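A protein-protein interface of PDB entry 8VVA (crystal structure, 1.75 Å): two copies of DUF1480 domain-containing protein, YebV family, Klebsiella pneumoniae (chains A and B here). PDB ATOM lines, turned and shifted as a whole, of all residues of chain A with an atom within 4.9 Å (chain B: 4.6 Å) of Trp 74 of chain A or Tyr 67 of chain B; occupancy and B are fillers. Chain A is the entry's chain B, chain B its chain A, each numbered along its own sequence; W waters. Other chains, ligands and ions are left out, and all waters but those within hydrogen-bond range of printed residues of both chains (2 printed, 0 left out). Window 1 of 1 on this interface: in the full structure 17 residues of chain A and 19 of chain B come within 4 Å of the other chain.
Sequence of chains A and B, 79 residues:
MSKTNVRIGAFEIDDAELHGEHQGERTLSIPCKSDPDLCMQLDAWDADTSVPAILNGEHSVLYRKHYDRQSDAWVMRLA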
ATOM      1  N   LEU A  28      -1.779  21.699 -13.017  1.00  0.00           N
ATOM      2  CA  LEU A  28      -3.015  22.382 -13.356  1.00  0.00           C
ATOM      3  C   LEU A  28      -3.925  22.332 -12.140  1.00  0.00           C
ATOM      4  O   LEU A  28      -3.833  21.413 -11.321  1.00  0.00           O
ATOM      5  CB  LEU A  28      -3.683  21.773 -14.597  1.00  0.00           C
ATOM      6  CG  LEU A  28      -4.437  20.445 -14.540  1.00  0.00           C
ATOM      7  CD1 LEU A  28      -5.860  20.619 -14.042  1.00  0.00           C
ATOM      8  CD2 LEU A  28      -4.469  19.800 -15.926  1.00  0.00           C
ATOM      9  N   SER A  29      -4.778  23.342 -12.017  1.00  0.00           N
ATOM     10  CA  SER A  29      -5.661  23.493 -10.868  1.00  0.00           C
ATOM     11  C   SER A  29      -7.102  23.317 -11.315  1.00  0.00           C
ATOM     12  O   SER A  29      -7.517  23.898 -12.325  1.00  0.00           O
ATOM     13  CB  SER A  29      -5.490  24.868 -10.213  1.00  0.00           C
ATOM     14  OG  SER A  29      -4.229  24.975  -9.562  1.00  0.00           O
ATOM     15  N   ILE A  30      -7.852  22.518 -10.568  1.00  0.00           N
ATOM     16  CA  ILE A  30      -9.273  22.282 -10.818  1.00  0.00           C
ATOM     17  C   ILE A  30     -10.073  23.008  -9.743  1.00  0.00           C
ATOM     18  O   ILE A  30      -9.950  22.667  -8.555  1.00  0.00           O
ATOM     19  CB  ILE A  30      -9.599  20.783 -10.825  1.00  0.00           C
ATOM     20  CG1 ILE A  30      -8.832  20.083 -11.943  1.00  0.00           C
ATOM     21  CG2 ILE A  30     -11.112  20.581 -10.951  1.00  0.00           C
ATOM     22  CD1 ILE A  30      -8.634  18.596 -11.677  1.00  0.00           C
ATOM     23  N   CYS A  32     -12.785  23.742  -7.260  1.00  0.00           N
ATOM     24  CA  CYS A  32     -13.825  22.912  -6.672  1.00  0.00           C
ATOM     25  C   CYS A  32     -15.135  23.667  -6.469  1.00  0.00           C
ATOM     26  O   CYS A  32     -16.184  23.026  -6.367  1.00  0.00           O
ATOM     27  CB  CYS A  32     -13.319  22.326  -5.358  1.00  0.00           C
ATOM     28  SG  CYS A  32     -11.883  21.226  -5.639  1.00  0.00           S
ATOM     29  N   CYS A  39     -14.264  17.256  -7.956  1.00  0.00           N
ATOM     30  CA  CYS A  39     -13.411  17.337  -6.776  1.00  0.00           C
ATOM     31  C   CYS A  39     -13.771  16.274  -5.749  1.00  0.00           C
ATOM     32  O   CYS A  39     -12.879  15.702  -5.117  1.00  0.00           O
ATOM     33  CB  CYS A  39     -13.467  18.734  -6.158  1.00  0.00           C
ATOM     34  SG  CYS A  39     -12.495  19.932  -7.121  1.00  0.00           S
ATOM     35  N   LEU A  42     -12.148  13.198  -6.850  1.00  0.00           N
ATOM     36  CA  LEU A  42     -10.711  13.280  -6.597  1.00  0.00           C
ATOM     37  C   LEU A  42     -10.404  13.058  -5.121  1.00  0.00           C
ATOM     38  O   LEU A  42      -9.396  12.439  -4.783  1.00  0.00           O
ATOM     39  CB  LEU A  42     -10.153  14.622  -7.074  1.00  0.00           C
ATOM     40  CG  LEU A  42     -10.186  14.803  -8.598  1.00  0.00           C
ATOM     41  CD1 LEU A  42      -9.836  16.229  -8.994  1.00  0.00           C
ATOM     42  CD2 LEU A  42      -9.249  13.795  -9.265  1.00  0.00           C
ATOM     43  N   ASP A  43     -11.279  13.531  -4.230  1.00  0.00           N
ATOM     44  CA  ASP A  43     -11.077  13.306  -2.798  1.00  0.00           C
ATOM     45  C   ASP A  43     -11.058  11.818  -2.477  1.00  0.00           C
ATOM     46  O   ASP A  43     -10.253  11.355  -1.656  1.00  0.00           O
ATOM     47  CB  ASP A  43     -12.189  13.968  -1.986  1.00  0.00           C
ATOM     48  CG  ASP A  43     -12.001  15.473  -1.814  1.00  0.00           C
ATOM     49  OD1 ASP A  43     -11.030  16.073  -2.343  1.00  0.00           O
ATOM     50  OD2 ASP A  43     -12.845  16.049  -1.101  1.00  0.00           O
ATOM     51  N   ALA A  44     -11.948  11.059  -3.101  1.00  0.00           N
ATOM     52  CA  ALA A  44     -12.092   9.646  -2.789  1.00  0.00           C
ATOM     53  C   ALA A  44     -11.230   8.760  -3.677  1.00  0.00           C
ATOM     54  O   ALA A  44     -11.278   7.535  -3.531  1.00  0.00           O
ATOM     55  CB  ALA A  44     -13.565   9.232  -2.904  1.00  0.00           C
ATOM     56  N   ARG A  64      -2.596  13.471  -8.172  1.00  0.00           N
ATOM     57  CA  ARG A  64      -3.001  14.431  -7.155  1.00  0.00           C
ATOM     58  C   ARG A  64      -1.767  14.941  -6.426  1.00  0.00           C
ATOM     59  O   ARG A  64      -0.963  14.154  -5.901  1.00  0.00           O
ATOM     60  CB  ARG A  64      -3.975  13.802  -6.167  1.00  0.00           C
ATOM     61  CG  ARG A  64      -5.218  13.191  -6.830  1.00  0.00           C
ATOM     62  CD  ARG A  64      -6.177  12.643  -5.758  1.00  0.00           C
ATOM     63  NE  ARG A  64      -5.496  11.701  -4.874  1.00  0.00           N
ATOM     64  CZ  ARG A  64      -5.976  11.261  -3.713  1.00  0.00           C
ATOM     65  NH1 ARG A  64      -7.163  11.663  -3.271  1.00  0.00           N
ATOM     66  NH2 ARG A  64      -5.258  10.414  -2.983  1.00  0.00           N
ATOM     67  N   LYS A  65      -1.618  16.257  -6.390  1.00  0.00           N
ATOM     68  CA  LYS A  65      -0.463  16.877  -5.746  1.00  0.00           C
ATOM     69  C   LYS A  65      -0.811  17.473  -4.387  1.00  0.00           C
ATOM     70  O   LYS A  65      -0.189  17.128  -3.376  1.00  0.00           O
ATOM     71  CB  LYS A  65       0.125  17.964  -6.654  1.00  0.00           C
ATOM     72  CG  LYS A  65       1.270  18.727  -6.003  1.00  0.00           C
ATOM     73  CD  LYS A  65       1.909  19.769  -6.910  1.00  0.00           C
ATOM     74  CE  LYS A  65       3.007  20.477  -6.127  1.00  0.00           C
ATOM     75  NZ  LYS A  65       4.012  21.082  -7.011  1.00  0.00           N
ATOM     76  N   HIS A  66      -1.828  18.331  -4.338  1.00  0.00           N
ATOM     77  CA  HIS A  66      -2.109  19.118  -3.148  1.00  0.00           C
ATOM     78  C   HIS A  66      -3.513  19.686  -3.265  1.00  0.00           C
ATOM     79  O   HIS A  66      -3.884  20.166  -4.332  1.00  0.00           O
ATOM     80  CB  HIS A  66      -1.094  20.269  -3.019  1.00  0.00           C
ATOM     81  CG  HIS A  66      -1.331  21.162  -1.840  1.00  0.00           C
ATOM     82  ND1 HIS A  66      -1.089  20.761  -0.544  1.00  0.00           N
ATOM     83  CD2 HIS A  66      -1.773  22.439  -1.761  1.00  0.00           C
ATOM     84  CE1 HIS A  66      -1.386  21.747   0.286  1.00  0.00           C
ATOM     85  NE2 HIS A  66      -1.799  22.779  -0.428  1.00  0.00           N
ATOM     86  N   TYR A  67      -4.277  19.667  -2.172  1.00  0.00           N
ATOM     87  CA  TYR A  67      -5.510  20.442  -2.120  1.00  0.00           C
ATOM     88  C   TYR A  67      -5.195  21.854  -1.626  1.00  0.00           C
ATOM     89  O   TYR A  67      -4.758  22.029  -0.481  1.00  0.00           O
ATOM     90  CB  TYR A  67      -6.570  19.815  -1.216  1.00  0.00           C
ATOM     91  CG  TYR A  67      -7.885  20.486  -1.500  1.00  0.00           C
ATOM     92  CD1 TYR A  67      -8.684  20.043  -2.536  1.00  0.00           C
ATOM     93  CD2 TYR A  67      -8.284  21.630  -0.809  1.00  0.00           C
ATOM     94  CE1 TYR A  67      -9.870  20.695  -2.856  1.00  0.00           C
ATOM     95  CE2 TYR A  67      -9.478  22.288  -1.122  1.00  0.00           C
ATOM     96  CZ  TYR A  67     -10.262  21.811  -2.146  1.00  0.00           C
ATOM     97  OH  TYR A  67     -11.440  22.442  -2.496  1.00  0.00           O
ATOM     98  N   ASP A  72      -9.536  26.777  -2.908  1.00  0.00           N
ATOM     99  CA  ASP A  72     -10.458  25.641  -3.004  1.00  0.00           C
ATOM    100  C   ASP A  72     -10.311  24.936  -4.353  1.00  0.00           C
ATOM    101  O   ASP A  72     -11.247  24.852  -5.151  1.00  0.00           O
ATOM    102  CB  ASP A  72     -11.905  26.096  -2.775  1.00  0.00           C
ATOM    103  CG  ASP A  72     -12.222  26.335  -1.302  1.00  0.00           C
ATOM    104  OD1 ASP A  72     -11.378  26.005  -0.451  1.00  0.00           O
ATOM    105  OD2 ASP A  72     -13.346  26.833  -1.010  1.00  0.00           O
ATOM    106  N   ALA A  73      -9.106  24.414  -4.595  1.00  0.00           N
ATOM    107  CA  ALA A  73      -8.805  23.820  -5.888  1.00  0.00           C
ATOM    108  C   ALA A  73      -7.927  22.594  -5.692  1.00  0.00           C
ATOM    109  O   ALA A  73      -7.064  22.588  -4.808  1.00  0.00           O
ATOM    110  CB  ALA A  73      -8.105  24.837  -6.808  1.00  0.00           C
ATOM    111  N   TRP A  74      -8.166  21.551  -6.488  1.00  0.00           N
ATOM    112  CA  TRP A  74      -7.240  20.424  -6.560  1.00  0.00           C
ATOM    113  C   TRP A  74      -6.089  20.776  -7.490  1.00  0.00           C
ATOM    114  O   TRP A  74      -6.307  21.111  -8.663  1.00  0.00           O
ATOM    115  CB  TRP A  74      -7.940  19.158  -7.063  1.00  0.00           C
ATOM    116  CG  TRP A  74      -8.268  18.233  -5.938  1.00  0.00           C
ATOM    117  CD1 TRP A  74      -9.512  17.901  -5.486  1.00  0.00           C
ATOM    118  CD2 TRP A  74      -7.339  17.520  -5.119  1.00  0.00           C
ATOM    119  NE1 TRP A  74      -9.413  17.037  -4.431  1.00  0.00           N
ATOM    120  CE2 TRP A  74      -8.087  16.787  -4.183  1.00  0.00           C
ATOM    121  CE3 TRP A  74      -5.936  17.435  -5.086  1.00  0.00           C
ATOM    122  CZ2 TRP A  74      -7.496  15.979  -3.221  1.00  0.00           C
ATOM    123  CZ3 TRP A  74      -5.342  16.628  -4.113  1.00  0.00           C
ATOM    124  CH2 TRP A  74      -6.121  15.908  -3.204  1.00  0.00           C
ATOM    125  N   VAL A  75      -4.866  20.724  -6.976  1.00  0.00           N
ATOM    126  CA  VAL A  75      -3.692  20.951  -7.805  1.00  0.00           C
ATOM    127  C   VAL A  75      -3.181  19.591  -8.229  1.00  0.00           C
ATOM    128  O   VAL A  75      -2.922  18.726  -7.381  1.00  0.00           O
ATOM    129  CB  VAL A  75      -2.607  21.745  -7.063  1.00  0.00           C
ATOM    130  CG1 VAL A  75      -1.509  22.091  -8.045  1.00  0.00           C
ATOM    131  CG2 VAL A  75      -3.222  22.997  -6.436  1.00  0.00           C
ATOM    132  N   MET A  76      -3.072  19.396  -9.540  1.00  0.00           N
ATOM    133  CA  MET A  76      -2.674  18.116 -10.110  1.00  0.00           C
ATOM    134  C   MET A  76      -1.327  18.259 -10.793  1.00  0.00           C
ATOM    135  O   MET A  76      -1.057  19.305 -11.376  1.00  0.00           O
ATOM    136  CB  MET A  76      -3.687  17.629 -11.147  1.00  0.00           C
ATOM    137  CG  MET A  76      -5.141  17.795 -10.764  1.00  0.00           C
ATOM    138  SD  MET A  76      -5.558  16.597  -9.323  1.00  0.00           S
ATOM    139  CE  MET A  76      -5.430  14.914 -10.323  1.00  0.00           C
ATOM    140  N   CYS B  32     -12.996  10.582   3.447  1.00  0.00           N
ATOM    141  CA  CYS B  32     -13.780  10.935   2.268  1.00  0.00           C
ATOM    142  C   CYS B  32     -14.218   9.733   1.437  1.00  0.00           C
ATOM    143  O   CYS B  32     -15.160   9.863   0.655  1.00  0.00           O
ATOM    144  CB  CYS B  32     -12.997  11.903   1.395  1.00  0.00           C
ATOM    145  SG  CYS B  32     -12.632  13.429   2.295  1.00  0.00           S
ATOM    146  N   HIS B  66      -5.685  20.283   6.360  1.00  0.00           N
ATOM    147  CA  HIS B  66      -4.900  19.607   5.339  1.00  0.00           C
ATOM    148  C   HIS B  66      -5.731  18.476   4.756  1.00  0.00           C
ATOM    149  O   HIS B  66      -6.395  17.760   5.505  1.00  0.00           O
ATOM    150  CB  HIS B  66      -3.605  19.059   5.964  1.00  0.00           C
ATOM    151  CG  HIS B  66      -2.783  18.215   5.045  1.00  0.00           C
ATOM    152  ND1 HIS B  66      -2.063  18.741   3.991  1.00  0.00           N
ATOM    153  CD2 HIS B  66      -2.555  16.881   5.028  1.00  0.00           C
ATOM    154  CE1 HIS B  66      -1.435  17.763   3.358  1.00  0.00           C
ATOM    155  NE2 HIS B  66      -1.714  16.627   3.967  1.00  0.00           N
ATOM    156  N   TYR B  67      -5.700  18.316   3.428  1.00  0.00           N
ATOM    157  CA  TYR B  67      -6.259  17.120   2.802  1.00  0.00           C
ATOM    158  C   TYR B  67      -5.185  16.038   2.734  1.00  0.00           C
ATOM    159  O   TYR B  67      -4.154  16.217   2.072  1.00  0.00           O
ATOM    160  CB  TYR B  67      -6.823  17.380   1.400  1.00  0.00           C
ATOM    161  CG  TYR B  67      -7.620  16.178   1.010  1.00  0.00           C
ATOM    162  CD1 TYR B  67      -8.910  16.031   1.482  1.00  0.00           C
ATOM    163  CD2 TYR B  67      -7.051  15.115   0.291  1.00  0.00           C
ATOM    164  CE1 TYR B  67      -9.648  14.897   1.214  1.00  0.00           C
ATOM    165  CE2 TYR B  67      -7.797  13.960   0.014  1.00  0.00           C
ATOM    166  CZ  TYR B  67      -9.102  13.880   0.481  1.00  0.00           C
ATOM    167  OH  TYR B  67      -9.890  12.765   0.245  1.00  0.00           O
ATOM    168  N   ASP B  68      -5.426  14.922   3.419  1.00  0.00           N
ATOM    169  CA  ASP B  68      -4.460  13.827   3.522  1.00  0.00           C
ATOM    170  C   ASP B  68      -4.657  12.870   2.350  1.00  0.00           C
ATOM    171  O   ASP B  68      -5.607  12.082   2.339  1.00  0.00           O
ATOM    172  CB  ASP B  68      -4.638  13.119   4.866  1.00  0.00           C
ATOM    173  CG  ASP B  68      -3.595  12.045   5.129  1.00  0.00           C
ATOM    174  OD1 ASP B  68      -2.986  11.521   4.177  1.00  0.00           O
ATOM    175  OD2 ASP B  68      -3.393  11.722   6.319  1.00  0.00           O
ATOM    176  N   ARG B  69      -3.737  12.908   1.379  1.00  0.00           N
ATOM    177  CA  ARG B  69      -3.867  12.061   0.196  1.00  0.00           C
ATOM    178  C   ARG B  69      -3.635  10.585   0.494  1.00  0.00           C
ATOM    179  O   ARG B  69      -4.134   9.734  -0.248  1.00  0.00           O
ATOM    180  CB  ARG B  69      -2.895  12.520  -0.892  1.00  0.00           C
ATOM    181  CG  ARG B  69      -3.261  13.834  -1.530  1.00  0.00           C
ATOM    182  CD  ARG B  69      -2.247  14.240  -2.618  1.00  0.00           C
ATOM    183  NE  ARG B  69      -0.920  14.514  -2.076  1.00  0.00           N
ATOM    184  CZ  ARG B  69       0.155  13.773  -2.312  1.00  0.00           C
ATOM    185  NH1 ARG B  69       0.075  12.683  -3.081  1.00  0.00           N
ATOM    186  NH2 ARG B  69       1.314  14.113  -1.767  1.00  0.00           N
ATOM    187  N   ASP B  72      -7.025   9.587   2.236  1.00  0.00           N
ATOM    188  CA  ASP B  72      -8.211  10.214   1.622  1.00  0.00           C
ATOM    189  C   ASP B  72      -9.133  10.805   2.692  1.00  0.00           C
ATOM    190  O   ASP B  72     -10.289  10.409   2.850  1.00  0.00           O
ATOM    191  CB  ASP B  72      -8.966   9.214   0.746  1.00  0.00           C
ATOM    192  CG  ASP B  72      -8.348   9.066  -0.624  1.00  0.00           C
ATOM    193  OD1 ASP B  72      -7.383   9.800  -0.936  1.00  0.00           O
ATOM    194  OD2 ASP B  72      -8.858   8.223  -1.387  1.00  0.00           O
ATOM    195  N   ALA B  73      -8.592  11.754   3.450  1.00  0.00           N
ATOM    196  CA  ALA B  73      -9.345  12.312   4.561  1.00  0.00           C
ATOM    197  C   ALA B  73      -9.096  13.805   4.685  1.00  0.00           C
ATOM    198  O   ALA B  73      -7.976  14.280   4.483  1.00  0.00           O
ATOM    199  CB  ALA B  73      -8.980  11.638   5.887  1.00  0.00           C
ATOM    200  N   TRP B  74     -10.144  14.537   5.046  1.00  0.00           N
ATOM    201  CA  TRP B  74      -9.989  15.930   5.438  1.00  0.00           C
ATOM    202  C   TRP B  74      -9.521  15.955   6.880  1.00  0.00           C
ATOM    203  O   TRP B  74     -10.205  15.430   7.764  1.00  0.00           O
ATOM    204  CB  TRP B  74     -11.309  16.696   5.293  1.00  0.00           C
ATOM    205  CG  TRP B  74     -11.341  17.506   4.064  1.00  0.00           C
ATOM    206  CD1 TRP B  74     -12.128  17.314   2.969  1.00  0.00           C
ATOM    207  CD2 TRP B  74     -10.498  18.626   3.770  1.00  0.00           C
ATOM    208  NE1 TRP B  74     -11.830  18.249   2.008  1.00  0.00           N
ATOM    209  CE2 TRP B  74     -10.841  19.073   2.481  1.00  0.00           C
ATOM    210  CE3 TRP B  74      -9.490  19.295   4.478  1.00  0.00           C
ATOM    211  CZ2 TRP B  74     -10.214  20.160   1.877  1.00  0.00           C
ATOM    212  CZ3 TRP B  74      -8.864  20.371   3.880  1.00  0.00           C
ATOM    213  CH2 TRP B  74      -9.225  20.795   2.593  1.00  0.00           C
HETATM  214  O   HOH W   1      -4.482  20.561   1.937  1.00  0.00           O
HETATM  215  O   HOH W   2      -3.259  18.089   0.093  1.00  0.00           O
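Of the 8 printed residues of chain B, 5 touch a printed residue of chain A.
Printed residues of chain B that touch a printed residue of chain A: Cys 32, Tyr 67, Arg 69, Asp 72 and Trp 74.
Hydrophobic or aromatic side chains of chain B that line the printed part of chain A: Tyr 67 and Trp 74.
Of the 17 printed residues of chain A, 6 touch a printed residue of chain B.
Printed residues of chain A that touch a printed residue of chain B: Asp 43, Ala 44, Arg 64, Lys 65, Tyr 67 and Trp 74.
Hydrophobic or aromatic side chains of chain A within 4 Å of the printed part of chain B: Ala 44, Tyr 67 and Trp 74.
The backbone carbonyl oxygen (O) of Arg 69 of chain B lies within hydrogen-bond range of the guanidinium group (NH2) of Arg 64 of chain A (3.0 Å).
The guanidinium group (NE) of Arg 69 of chain B lies within hydrogen-bond range of the backbone carbonyl oxygen (O) of Lys 65 of chain A (3.0 Å).
OD1 of Asp 72 of chain B lies within salt-bridge range of NH1 of Arg 64 of chain A, at 3.0 Å.
The backbone carbonyl oxygen of Asp 43 of chain A sits close to the side-chain hydroxyl of Tyr 67 of chain B, at 2.4 Å.
The side-chain carboxylate (OD1) of Asp 72 of chain B lies close to the backbone carbonyl oxygen (O) of Asp 43 of chain A (3.3 Å).
OD2 of Asp 72 of chain B sits close to O of Ala 44 of chain A (3.3 Å).
The side-chain hydroxyl (OH) of Tyr 67 of chain B lies close to the side-chain sulfur (SG) of Cys 32 of chain B (3.5 Å).
N of Cys 32 of chain B is in hydrogen-bond range of O of Asp 72 of chain B (2.8 Å).
The backbone carbonyl oxygen of Trp 74 of chain A is in hydrogen-bond range of the backbone NH of Ile 30 of chain A (2.8 Å).
The backbone carbonyl oxygen of Leu 42 of chain A is in hydrogen-bond range of the guanidinium group of Arg 64 of chain A, at 2.8 Å.
NE1 of Trp 74 of chain A lies within hydrogen-bond range of OD1 of Asp 43 of chain A (2.8 Å).
The backbone carbonyl oxygen (O) of Val 75 of chain A is in hydrogen-bond range of the backbone NH (N) of Lys 65 of chain A, 3.0 Å away.
Water W1 lies within hydrogen-bond range of the backbone carbonyl oxygen of Tyr 67 of chain A (2.8 Å) and the backbone NH of Tyr 67 of chain B (3.0 Å).
Water W2 bridges the backbone carbonyl oxygen (O) of Tyr 67 of chain B and the backbone NH (N) of Tyr 67 of chain A.
Trp 74 of chain B touches Asp 43 of chain A (NE1 to OD2, 3.9 Å).
Cys 32 of chain B touches Ala 44 of chain A (O to CB, 3.95 Å).
Tyr 67 of chain B touches Tyr 67 of chain A (CB to CB, 3.6 Å).
CZ2 of Trp 74 of chain B touches CD2 of Tyr 67 of chain A, 3.6 Å away.
Tyr 67 of chain B touches Trp 74 of chain A.
Trp 74 of chain A touches Arg 69 of chain B (CH2 to CG, 3.9 Å).
Tyr 67 of chain B touches its own counterpart, Tyr 67 of chain A.
Tyr 67 of chain A touches Trp 74 of chain B, and with the chains exchanged Trp 74 of chain A touches Tyr 67 of chain B.
Positions printed for both chains: 32, 66, 67, 72, 73 and 74.
Ser 29 of chain A touches none of the printed residues of chain B.
Of the printed residues of chain B, Ala 44 of chain A touches Cys 32 and Asp 72.
Printed residues of chain B within 4 Å of Lys 65 of chain A: Arg 69 (3.0 Å).
Of the printed residues of chain B, Tyr 67 of chain A touches Tyr 67 (3.6 Å) and Trp 74 (3.6 Å).
Trp 74 of chain A touches just these residues of chain B: Tyr 67 (3.6 Å) and Arg 69 (3.9 Å).
Of chain A, only Asp 43 (2.4 Å), Tyr 67 (3.6 Å) and Trp 74 (3.6 Å) come within 4 Å of Tyr 67 of chain B.
Ala 73 of chain B touches none of the printed residues of chain A.
The nearest printed residue of chain B that does not touch Trp 74 of chain A is Asp 68 of chain B (6.5 Å).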
